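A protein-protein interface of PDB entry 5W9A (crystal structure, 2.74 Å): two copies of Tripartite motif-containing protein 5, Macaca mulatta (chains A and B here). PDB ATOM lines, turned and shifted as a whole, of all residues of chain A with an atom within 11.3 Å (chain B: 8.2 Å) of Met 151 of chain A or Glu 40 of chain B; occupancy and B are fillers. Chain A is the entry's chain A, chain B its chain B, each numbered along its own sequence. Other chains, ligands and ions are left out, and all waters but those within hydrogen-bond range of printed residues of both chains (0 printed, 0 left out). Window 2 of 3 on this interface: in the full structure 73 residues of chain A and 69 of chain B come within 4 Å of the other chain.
Among the printed residues, merely in contact across the chains: Leu 155 of chain A with Phe 13 of chain B, Val 158 of chain A with Tyr 46 of chain B, Leu 155 of chain A with Met 39 of chain B, Leu 155 of chain A with Tyr 46 of chain B, Met 152 of chain A with Val 20 of chain B, Leu 154 of chain A with Tyr 46 of chain B, Met 151 of chain A with Glu 40 of chain B, Met 151 of chain A with Ala 43 of chain B and Val 158 of chain A with Phe 13 of chain B.
The side-chain carboxylate (OD1) of Asp 159 of chain A is in hydrogen-bond range of the side-chain hydroxyl (OH) of Tyr 46 of chain B (3.3 Å). The backbone carbonyl oxygen (O) of Met 39 of chain B sits close to the side-chain sulfur (SD) of Met 151 of chain A (3.8 Å). N of Val 20 of chain B is in hydrogen-bond range of OE1 of Gln 156 of chain A, 3.0 Å away.
Glu 40 of chain B touches one residue of chain A. No residue of chain B comes within 4 Å of Ser 150 of chain A. Met 39 of chain B touches two residues of chain A. No residue of chain A comes within 4 Å of Glu 41 of chain B. Ala 43 of chain B touches just one residue of chain A: Met 151 (3.8 Å). Of the printed residues of chain B, Asp 159 of chain A touches Tyr 46. Of the printed residues of chain B, Val 158 of chain A touches Phe 13 (3.99 Å) and Tyr 46 (3.5 Å). Of the printed residues of chain A, Phe 13 of chain B touches Leu 155 and Val 158. The nearest residue of chain B that does not touch Met 151 of chain A is Val 20 of chain B (5.7 Å). The nearest residue of chain A that does not touch Glu 40 of chain B is Leu 155 of chain A (5.4 Å).
Of the 17 printed residues of chain A, 7 touch a printed residue of chain B. Printed residues of chain A that touch a printed residue of chain B: Met 151, Met 152, Leu 154, Leu 155, Gln 156, Val 158 and Asp 159. Hydrophobic or aromatic side chains of chain A that line the printed part of chain B: Met 151, Met 152, Leu 154, Leu 155 and Val 158. Of the 15 printed residues of chain B, 6 touch a printed residue of chain A. Hydrophobic or aromatic side chains of chain B that line the printed part of chain A: Phe 13, Val 20, Met 39, Ala 43 and Tyr 46. Among the printed residues, no Asp or Glu carboxylate lies within 4 Å of a Lys or Arg side-chain nitrogen of the other chain.
No position is printed for both chains.
The backbone NH of Met 152 of chain A sits close to the side-chain hydroxyl of Ser 150 of chain A. NH2 of Arg 146 of chain A sits at hydrogen-bond distance from O of Gln 156 of chain A (2.9 Å). O of Leu 154 of chain A is in hydrogen-bond range of NH1 of Arg 146 of chain A. The backbone carbonyl oxygen (O) of Phe 37 of chain B sits at hydrogen-bond distance from the backbone NH (N) of Phe 13 of chain B (2.9 Å). The backbone carbonyl oxygen (O) of Leu 11 of chain B lies within hydrogen-bond range of the backbone NH (N) of Met 39 of chain B (3.5 Å).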
ATOM      1  N   LEU A 143      -6.867  -3.118 -12.820  1.00  0.00           N
ATOM      2  CA  LEU A 143      -5.484  -3.470 -12.511  1.00  0.00           C
ATOM      3  C   LEU A 143      -4.927  -4.483 -13.506  1.00  0.00           C
ATOM      4  O   LEU A 143      -3.746  -4.420 -13.865  1.00  0.00           O
ATOM      5  CB  LEU A 143      -5.371  -4.001 -11.082  1.00  0.00           C
ATOM      6  CG  LEU A 143      -5.398  -2.937  -9.984  1.00  0.00           C
ATOM      7  CD1 LEU A 143      -4.881  -3.513  -8.678  1.00  0.00           C
ATOM      8  CD2 LEU A 143      -4.581  -1.721 -10.396  1.00  0.00           C
ATOM      9  N   GLU A 144      -5.752  -5.432 -13.953  1.00  0.00           N
ATOM     10  CA  GLU A 144      -5.305  -6.369 -14.982  1.00  0.00           C
ATOM     11  C   GLU A 144      -4.919  -5.629 -16.260  1.00  0.00           C
ATOM     12  O   GLU A 144      -3.847  -5.868 -16.837  1.00  0.00           O
ATOM     13  CB  GLU A 144      -6.395  -7.403 -15.259  1.00  0.00           C
ATOM     14  CG  GLU A 144      -6.636  -8.366 -14.107  1.00  0.00           C
ATOM     15  CD  GLU A 144      -7.843  -9.252 -14.331  1.00  0.00           C
ATOM     16  OE1 GLU A 144      -8.617  -8.977 -15.271  1.00  0.00           O
ATOM     17  OE2 GLU A 144      -8.019 -10.224 -13.566  1.00  0.00           O
ATOM     18  N   HIS A 145      -5.792  -4.723 -16.714  1.00  0.00           N
ATOM     19  CA  HIS A 145      -5.476  -3.917 -17.890  1.00  0.00           C
ATOM     20  C   HIS A 145      -4.206  -3.103 -17.672  1.00  0.00           C
ATOM     21  O   HIS A 145      -3.418  -2.904 -18.605  1.00  0.00           O
ATOM     22  CB  HIS A 145      -6.648  -2.997 -18.228  1.00  0.00           C
ATOM     23  CG  HIS A 145      -6.351  -2.022 -19.324  1.00  0.00           C
ATOM     24  ND1 HIS A 145      -5.728  -0.813 -19.098  1.00  0.00           N
ATOM     25  CD2 HIS A 145      -6.580  -2.082 -20.657  1.00  0.00           C
ATOM     26  CE1 HIS A 145      -5.592  -0.167 -20.243  1.00  0.00           C
ATOM     27  NE2 HIS A 145      -6.101  -0.916 -21.205  1.00  0.00           N
ATOM     28  N   ARG A 146      -3.995  -2.617 -16.448  1.00  0.00           N
ATOM     29  CA  ARG A 146      -2.787  -1.857 -16.145  1.00  0.00           C
ATOM     30  C   ARG A 146      -1.545  -2.730 -16.269  1.00  0.00           C
ATOM     31  O   ARG A 146      -0.511  -2.285 -16.782  1.00  0.00           O
ATOM     32  CB  ARG A 146      -2.880  -1.267 -14.739  1.00  0.00           C
ATOM     33  CG  ARG A 146      -3.797  -0.062 -14.609  1.00  0.00           C
ATOM     34  CD  ARG A 146      -3.364   1.071 -15.511  1.00  0.00           C
ATOM     35  NE  ARG A 146      -4.235   2.236 -15.388  1.00  0.00           N
ATOM     36  CZ  ARG A 146      -3.999   3.262 -14.578  1.00  0.00           C
ATOM     37  NH1 ARG A 146      -2.917   3.269 -13.811  1.00  0.00           N
ATOM     38  NH2 ARG A 146      -4.846   4.281 -14.532  1.00  0.00           N
ATOM     39  N   LEU A 147      -1.628  -3.974 -15.797  1.00  0.00           N
ATOM     40  CA  LEU A 147      -0.475  -4.865 -15.791  1.00  0.00           C
ATOM     41  C   LEU A 147      -0.207  -5.511 -17.141  1.00  0.00           C
ATOM     42  O   LEU A 147       0.880  -6.071 -17.329  1.00  0.00           O
ATOM     43  CB  LEU A 147      -0.657  -5.973 -14.751  1.00  0.00           C
ATOM     44  CG  LEU A 147      -0.114  -5.730 -13.343  1.00  0.00           C
ATOM     45  CD1 LEU A 147      -0.863  -4.604 -12.681  1.00  0.00           C
ATOM     46  CD2 LEU A 147      -0.210  -6.998 -12.506  1.00  0.00           C
ATOM     47  N   GLN A 148      -1.149  -5.455 -18.080  1.00  0.00           N
ATOM     48  CA  GLN A 148      -0.915  -6.089 -19.373  1.00  0.00           C
ATOM     49  C   GLN A 148      -0.544  -5.114 -20.481  1.00  0.00           C
ATOM     50  O   GLN A 148       0.109  -5.520 -21.448  1.00  0.00           O
ATOM     51  CB  GLN A 148      -2.148  -6.892 -19.805  1.00  0.00           C
ATOM     52  CG  GLN A 148      -3.424  -6.078 -19.995  1.00  0.00           C
ATOM     53  CD  GLN A 148      -3.530  -5.449 -21.375  1.00  0.00           C
ATOM     54  OE1 GLN A 148      -2.850  -5.864 -22.314  1.00  0.00           O
ATOM     55  NE2 GLN A 148      -4.381  -4.438 -21.500  1.00  0.00           N
ATOM     56  N   GLY A 149      -0.932  -3.848 -20.374  1.00  0.00           N
ATOM     57  CA  GLY A 149      -0.813  -2.907 -21.473  1.00  0.00           C
ATOM     58  C   GLY A 149       0.511  -2.180 -21.546  1.00  0.00           C
ATOM     59  O   GLY A 149       1.554  -2.679 -21.111  1.00  0.00           O
ATOM     60  N   SER A 150       0.461  -0.974 -22.110  1.00  0.00           N
ATOM     61  CA  SER A 150       1.652  -0.176 -22.352  1.00  0.00           C
ATOM     62  C   SER A 150       2.213   0.379 -21.044  1.00  0.00           C
ATOM     63  O   SER A 150       1.591   0.310 -19.980  1.00  0.00           O
ATOM     64  CB  SER A 150       1.341   0.967 -23.317  1.00  0.00           C
ATOM     65  OG  SER A 150       2.479   1.786 -23.525  1.00  0.00           O
ATOM     66  N   MET A 151       3.421   0.942 -21.139  1.00  0.00           N
ATOM     67  CA  MET A 151       4.016   1.616 -19.992  1.00  0.00           C
ATOM     68  C   MET A 151       3.268   2.904 -19.667  1.00  0.00           C
ATOM     69  O   MET A 151       3.059   3.230 -18.493  1.00  0.00           O
ATOM     70  CB  MET A 151       5.493   1.902 -20.263  1.00  0.00           C
ATOM     71  CG  MET A 151       6.320   2.167 -19.014  1.00  0.00           C
ATOM     72  SD  MET A 151       8.081   2.312 -19.378  1.00  0.00           S
ATOM     73  CE  MET A 151       8.393   0.744 -20.186  1.00  0.00           C
ATOM     74  N   MET A 152       2.862   3.650 -20.698  1.00  0.00           N
ATOM     75  CA  MET A 152       2.065   4.851 -20.471  1.00  0.00           C
ATOM     76  C   MET A 152       0.713   4.502 -19.865  1.00  0.00           C
ATOM     77  O   MET A 152       0.222   5.208 -18.977  1.00  0.00           O
ATOM     78  CB  MET A 152       1.888   5.618 -21.782  1.00  0.00           C
ATOM     79  CG  MET A 152       1.087   6.902 -21.653  1.00  0.00           C
ATOM     80  N   ASP A 153       0.093   3.419 -20.339  1.00  0.00           N
ATOM     81  CA  ASP A 153      -1.120   2.920 -19.699  1.00  0.00           C
ATOM     82  C   ASP A 153      -0.867   2.579 -18.237  1.00  0.00           C
ATOM     83  O   ASP A 153      -1.687   2.892 -17.367  1.00  0.00           O
ATOM     84  CB  ASP A 153      -1.646   1.694 -20.447  1.00  0.00           C
ATOM     85  CG  ASP A 153      -2.209   2.039 -21.810  1.00  0.00           C
ATOM     86  OD1 ASP A 153      -2.798   3.131 -21.955  1.00  0.00           O
ATOM     87  OD2 ASP A 153      -2.066   1.214 -22.736  1.00  0.00           O
ATOM     88  N   LEU A 154       0.276   1.952 -17.948  1.00  0.00           N
ATOM     89  CA  LEU A 154       0.580   1.529 -16.586  1.00  0.00           C
ATOM     90  C   LEU A 154       0.788   2.724 -15.663  1.00  0.00           C
ATOM     91  O   LEU A 154       0.419   2.675 -14.485  1.00  0.00           O
ATOM     92  CB  LEU A 154       1.816   0.624 -16.592  1.00  0.00           C
ATOM     93  CG  LEU A 154       2.200  -0.166 -15.337  1.00  0.00           C
ATOM     94  CD1 LEU A 154       2.921  -1.444 -15.733  1.00  0.00           C
ATOM     95  CD2 LEU A 154       3.080   0.656 -14.405  1.00  0.00           C
ATOM     96  N   LEU A 155       1.376   3.804 -16.176  1.00  0.00           N
ATOM     97  CA  LEU A 155       1.796   4.908 -15.323  1.00  0.00           C
ATOM     98  C   LEU A 155       0.812   6.070 -15.278  1.00  0.00           C
ATOM     99  O   LEU A 155       0.851   6.848 -14.320  1.00  0.00           O
ATOM    100  CB  LEU A 155       3.169   5.428 -15.765  1.00  0.00           C
ATOM    101  CG  LEU A 155       4.321   4.463 -15.480  1.00  0.00           C
ATOM    102  CD1 LEU A 155       5.630   5.015 -16.005  1.00  0.00           C
ATOM    103  CD2 LEU A 155       4.416   4.171 -13.989  1.00  0.00           C
ATOM    104  N   GLN A 156      -0.058   6.217 -16.274  1.00  0.00           N
ATOM    105  CA  GLN A 156      -0.953   7.367 -16.307  1.00  0.00           C
ATOM    106  C   GLN A 156      -2.013   7.230 -15.221  1.00  0.00           C
ATOM    107  O   GLN A 156      -2.795   6.272 -15.222  1.00  0.00           O
ATOM    108  CB  GLN A 156      -1.606   7.498 -17.681  1.00  0.00           C
ATOM    109  CG  GLN A 156      -2.562   8.677 -17.802  1.00  0.00           C
ATOM    110  CD  GLN A 156      -1.930   9.993 -17.390  1.00  0.00           C
ATOM    111  OE1 GLN A 156      -0.763  10.256 -17.683  1.00  0.00           O
ATOM    112  NE2 GLN A 156      -2.699  10.828 -16.701  1.00  0.00           N
ATOM    113  N   GLY A 157      -2.042   8.190 -14.300  1.00  0.00           N
ATOM    114  CA  GLY A 157      -3.016   8.165 -13.223  1.00  0.00           C
ATOM    115  C   GLY A 157      -2.871   6.988 -12.285  1.00  0.00           C
ATOM    116  O   GLY A 157      -3.865   6.547 -11.697  1.00  0.00           O
ATOM    117  N   VAL A 158      -1.653   6.465 -12.125  1.00  0.00           N
ATOM    118  CA  VAL A 158      -1.462   5.284 -11.290  1.00  0.00           C
ATOM    119  C   VAL A 158      -1.601   5.640  -9.813  1.00  0.00           C
ATOM    120  O   VAL A 158      -2.115   4.846  -9.015  1.00  0.00           O
ATOM    121  CB  VAL A 158      -0.105   4.625 -11.601  1.00  0.00           C
ATOM    122  CG1 VAL A 158       1.038   5.602 -11.370  1.00  0.00           C
ATOM    123  CG2 VAL A 158       0.082   3.361 -10.775  1.00  0.00           C
ATOM    124  N   ASP A 159      -1.156   6.840  -9.426  1.00  0.00           N
ATOM    125  CA  ASP A 159      -1.279   7.252  -8.033  1.00  0.00           C
ATOM    126  C   ASP A 159      -2.737   7.405  -7.628  1.00  0.00           C
ATOM    127  O   ASP A 159      -3.089   7.137  -6.475  1.00  0.00           O
ATOM    128  CB  ASP A 159      -0.518   8.555  -7.795  1.00  0.00           C
ATOM    129  CG  ASP A 159       0.983   8.390  -7.945  1.00  0.00           C
ATOM    130  OD1 ASP A 159       1.480   7.264  -7.734  1.00  0.00           O
ATOM    131  OD2 ASP A 159       1.663   9.385  -8.271  1.00  0.00           O
ATOM    132  N   LEU B  10       5.655  11.825 -25.122  1.00  0.00           N
ATOM    133  CA  LEU B  10       5.397  11.632 -23.695  1.00  0.00           C
ATOM    134  C   LEU B  10       6.305  10.506 -23.213  1.00  0.00           C
ATOM    135  O   LEU B  10       5.920   9.337 -23.180  1.00  0.00           O
ATOM    136  CB  LEU B  10       3.928  11.321 -23.427  1.00  0.00           C
ATOM    137  CG  LEU B  10       2.894  12.386 -23.792  1.00  0.00           C
ATOM    138  CD1 LEU B  10       2.343  12.128 -25.179  1.00  0.00           C
ATOM    139  CD2 LEU B  10       1.774  12.430 -22.764  1.00  0.00           C
ATOM    140  N   LEU B  11       7.528  10.870 -22.835  1.00  0.00           N
ATOM    141  CA  LEU B  11       8.504   9.924 -22.317  1.00  0.00           C
ATOM    142  C   LEU B  11       8.796  10.140 -20.842  1.00  0.00           C
ATOM    143  O   LEU B  11       9.580   9.383 -20.258  1.00  0.00           O
ATOM    144  CB  LEU B  11       9.807  10.013 -23.121  1.00  0.00           C
ATOM    145  CG  LEU B  11       9.706   9.692 -24.612  1.00  0.00           C
ATOM    146  CD1 LEU B  11      11.012  10.014 -25.322  1.00  0.00           C
ATOM    147  CD2 LEU B  11       9.320   8.235 -24.821  1.00  0.00           C
ATOM    148  N   LEU B  12       8.190  11.147 -20.226  1.00  0.00           N
ATOM    149  CA  LEU B  12       8.464  11.521 -18.849  1.00  0.00           C
ATOM    150  C   LEU B  12       7.294  11.147 -17.948  1.00  0.00           C
ATOM    151  O   LEU B  12       6.198  10.813 -18.404  1.00  0.00           O
ATOM    152  CB  LEU B  12       8.758  13.022 -18.748  1.00  0.00           C
ATOM    153  CG  LEU B  12      10.057  13.490 -19.407  1.00  0.00           C
ATOM    154  CD1 LEU B  12      10.198  15.002 -19.313  1.00  0.00           C
ATOM    155  CD2 LEU B  12      11.250  12.795 -18.774  1.00  0.00           C
ATOM    156  N   PHE B  13       7.556  11.201 -16.645  1.00  0.00           N
ATOM    157  CA  PHE B  13       6.570  10.906 -15.615  1.00  0.00           C
ATOM    158  C   PHE B  13       6.788  11.867 -14.459  1.00  0.00           C
ATOM    159  O   PHE B  13       7.910  11.992 -13.954  1.00  0.00           O
ATOM    160  CB  PHE B  13       6.680   9.453 -15.137  1.00  0.00           C
ATOM    161  CG  PHE B  13       5.666   9.077 -14.093  1.00  0.00           C
ATOM    162  CD1 PHE B  13       4.356   8.800 -14.447  1.00  0.00           C
ATOM    163  CD2 PHE B  13       6.025   8.992 -12.758  1.00  0.00           C
ATOM    164  CE1 PHE B  13       3.422   8.451 -13.488  1.00  0.00           C
ATOM    165  CE2 PHE B  13       5.096   8.643 -11.795  1.00  0.00           C
ATOM    166  CZ  PHE B  13       3.792   8.372 -12.161  1.00  0.00           C
ATOM    167  N   VAL B  20       1.958  11.458 -17.298  1.00  0.00           N
ATOM    168  CA  VAL B  20       3.062  11.446 -18.250  1.00  0.00           C
ATOM    169  C   VAL B  20       3.003  12.713 -19.093  1.00  0.00           C
ATOM    170  O   VAL B  20       1.927  13.143 -19.528  1.00  0.00           O
ATOM    171  CB  VAL B  20       3.018  10.177 -19.122  1.00  0.00           C
ATOM    172  CG1 VAL B  20       3.292   8.947 -18.271  1.00  0.00           C
ATOM    173  CG2 VAL B  20       1.675  10.049 -19.821  1.00  0.00           C
ATOM    174  N   PHE B  37      10.828  12.200 -13.893  1.00  0.00           N
ATOM    175  CA  PHE B  37      11.687  11.054 -14.161  1.00  0.00           C
ATOM    176  C   PHE B  37      11.307  10.445 -15.505  1.00  0.00           C
ATOM    177  O   PHE B  37      10.366  10.885 -16.169  1.00  0.00           O
ATOM    178  CB  PHE B  37      11.582  10.002 -13.047  1.00  0.00           C
ATOM    179  CG  PHE B  37      12.089  10.472 -11.715  1.00  0.00           C
ATOM    180  CD1 PHE B  37      13.201  11.292 -11.632  1.00  0.00           C
ATOM    181  CD2 PHE B  37      11.454  10.091 -10.546  1.00  0.00           C
ATOM    182  CE1 PHE B  37      13.670  11.725 -10.407  1.00  0.00           C
ATOM    183  CE2 PHE B  37      11.919  10.520  -9.317  1.00  0.00           C
ATOM    184  CZ  PHE B  37      13.029  11.339  -9.248  1.00  0.00           C
ATOM    185  N   LEU B  38      12.056   9.426 -15.910  1.00  0.00           N
ATOM    186  CA  LEU B  38      11.711   8.641 -17.086  1.00  0.00           C
ATOM    187  C   LEU B  38      10.782   7.500 -16.689  1.00  0.00           C
ATOM    188  O   LEU B  38      10.837   6.992 -15.566  1.00  0.00           O
ATOM    189  CB  LEU B  38      12.964   8.088 -17.769  1.00  0.00           C
ATOM    190  CG  LEU B  38      13.702   9.022 -18.734  1.00  0.00           C
ATOM    191  CD1 LEU B  38      14.574  10.019 -17.982  1.00  0.00           C
ATOM    192  CD2 LEU B  38      14.533   8.223 -19.728  1.00  0.00           C
ATOM    193  N   MET B  39       9.912   7.112 -17.624  1.00  0.00           N
ATOM    194  CA  MET B  39       8.955   6.043 -17.351  1.00  0.00           C
ATOM    195  C   MET B  39       9.662   4.732 -17.027  1.00  0.00           C
ATOM    196  O   MET B  39       9.215   3.971 -16.155  1.00  0.00           O
ATOM    197  CB  MET B  39       8.020   5.865 -18.549  1.00  0.00           C
ATOM    198  CG  MET B  39       7.024   6.997 -18.739  1.00  0.00           C
ATOM    199  SD  MET B  39       5.797   6.640 -20.013  1.00  0.00           S
ATOM    200  CE  MET B  39       6.855   6.320 -21.423  1.00  0.00           C
ATOM    201  N   GLU B  40      10.775   4.456 -17.713  1.00  0.00           N
ATOM    202  CA  GLU B  40      11.486   3.198 -17.524  1.00  0.00           C
ATOM    203  C   GLU B  40      12.142   3.098 -16.154  1.00  0.00           C
ATOM    204  O   GLU B  40      12.485   1.991 -15.727  1.00  0.00           O
ATOM    205  CB  GLU B  40      12.543   3.025 -18.617  1.00  0.00           C
ATOM    206  CG  GLU B  40      11.981   2.878 -20.027  1.00  0.00           C
ATOM    207  CD  GLU B  40      11.624   4.210 -20.664  1.00  0.00           C
ATOM    208  OE1 GLU B  40      11.696   5.247 -19.971  1.00  0.00           O
ATOM    209  OE2 GLU B  40      11.274   4.221 -21.863  1.00  0.00           O
ATOM    210  N   GLU B  41      12.323   4.222 -15.457  1.00  0.00           N
ATOM    211  CA  GLU B  41      12.970   4.179 -14.151  1.00  0.00           C
ATOM    212  C   GLU B  41      12.022   3.657 -13.078  1.00  0.00           C
ATOM    213  O   GLU B  41      12.442   2.908 -12.189  1.00  0.00           O
ATOM    214  CB  GLU B  41      13.501   5.565 -13.782  1.00  0.00           C
ATOM    215  CG  GLU B  41      14.656   6.039 -14.656  1.00  0.00           C
ATOM    216  CD  GLU B  41      15.136   7.431 -14.291  1.00  0.00           C
ATOM    217  OE1 GLU B  41      14.394   8.153 -13.593  1.00  0.00           O
ATOM    218  OE2 GLU B  41      16.256   7.802 -14.703  1.00  0.00           O
ATOM    219  N   VAL B  42      10.747   4.040 -13.143  1.00  0.00           N
ATOM    220  CA  VAL B  42       9.754   3.653 -12.146  1.00  0.00           C
ATOM    221  C   VAL B  42       8.807   2.578 -12.656  1.00  0.00           C
ATOM    222  O   VAL B  42       7.881   2.178 -11.923  1.00  0.00           O
ATOM    223  CB  VAL B  42       8.959   4.876 -11.654  1.00  0.00           C
ATOM    224  CG1 VAL B  42       9.887   5.885 -10.994  1.00  0.00           C
ATOM    225  CG2 VAL B  42       8.211   5.517 -12.812  1.00  0.00           C
ATOM    226  N   ALA B  43       9.012   2.090 -13.883  1.00  0.00           N
ATOM    227  CA  ALA B  43       8.102   1.107 -14.464  1.00  0.00           C
ATOM    228  C   ALA B  43       8.028  -0.158 -13.615  1.00  0.00           C
ATOM    229  O   ALA B  43       6.936  -0.602 -13.246  1.00  0.00           O
ATOM    230  CB  ALA B  43       8.535   0.774 -15.893  1.00  0.00           C
ATOM    231  N   GLN B  44       9.182  -0.755 -13.300  1.00  0.00           N
ATOM    232  CA  GLN B  44       9.190  -2.019 -12.565  1.00  0.00           C
ATOM    233  C   GLN B  44       8.642  -1.851 -11.151  1.00  0.00           C
ATOM    234  O   GLN B  44       7.930  -2.732 -10.643  1.00  0.00           O
ATOM    235  CB  GLN B  44      10.606  -2.596 -12.522  1.00  0.00           C
ATOM    236  CG  GLN B  44      10.973  -3.453 -13.726  1.00  0.00           C
ATOM    237  CD  GLN B  44      11.047  -2.661 -15.016  1.00  0.00           C
ATOM    238  OE1 GLN B  44      11.514  -1.523 -15.035  1.00  0.00           O
ATOM    239  NE2 GLN B  44      10.582  -3.262 -16.106  1.00  0.00           N
ATOM    240  N   GLU B  45       8.977  -0.740 -10.494  1.00  0.00           N
ATOM    241  CA  GLU B  45       8.468  -0.487  -9.151  1.00  0.00           C
ATOM    242  C   GLU B  45       6.947  -0.412  -9.153  1.00  0.00           C
ATOM    243  O   GLU B  45       6.275  -1.089  -8.361  1.00  0.00           O
ATOM    244  CB  GLU B  45       9.082   0.799  -8.596  1.00  0.00           C
ATOM    245  CG  GLU B  45       8.554   1.212  -7.232  1.00  0.00           C
ATOM    246  CD  GLU B  45       9.140   2.530  -6.756  1.00  0.00           C
ATOM    247  OE1 GLU B  45       9.981   3.105  -7.480  1.00  0.00           O
ATOM    248  OE2 GLU B  45       8.762   2.988  -5.658  1.00  0.00           O
ATOM    249  N   TYR B  46       6.378   0.401 -10.050  1.00  0.00           N
ATOM    250  CA  TYR B  46       4.923   0.489 -10.107  1.00  0.00           C
ATOM    251  C   TYR B  46       4.302  -0.833 -10.544  1.00  0.00           C
ATOM    252  O   TYR B  46       3.198  -1.172 -10.102  1.00  0.00           O
ATOM    253  CB  TYR B  46       4.495   1.619 -11.043  1.00  0.00           C
ATOM    254  CG  TYR B  46       4.540   2.989 -10.403  1.00  0.00           C
ATOM    255  CD1 TYR B  46       3.484   3.446  -9.626  1.00  0.00           C
ATOM    256  CD2 TYR B  46       5.632   3.828 -10.582  1.00  0.00           C
ATOM    257  CE1 TYR B  46       3.519   4.697  -9.039  1.00  0.00           C
ATOM    258  CE2 TYR B  46       5.674   5.081 -10.000  1.00  0.00           C
ATOM    259  CZ  TYR B  46       4.614   5.511  -9.230  1.00  0.00           C
ATOM    260  OH  TYR B  46       4.649   6.757  -8.648  1.00  0.00           O
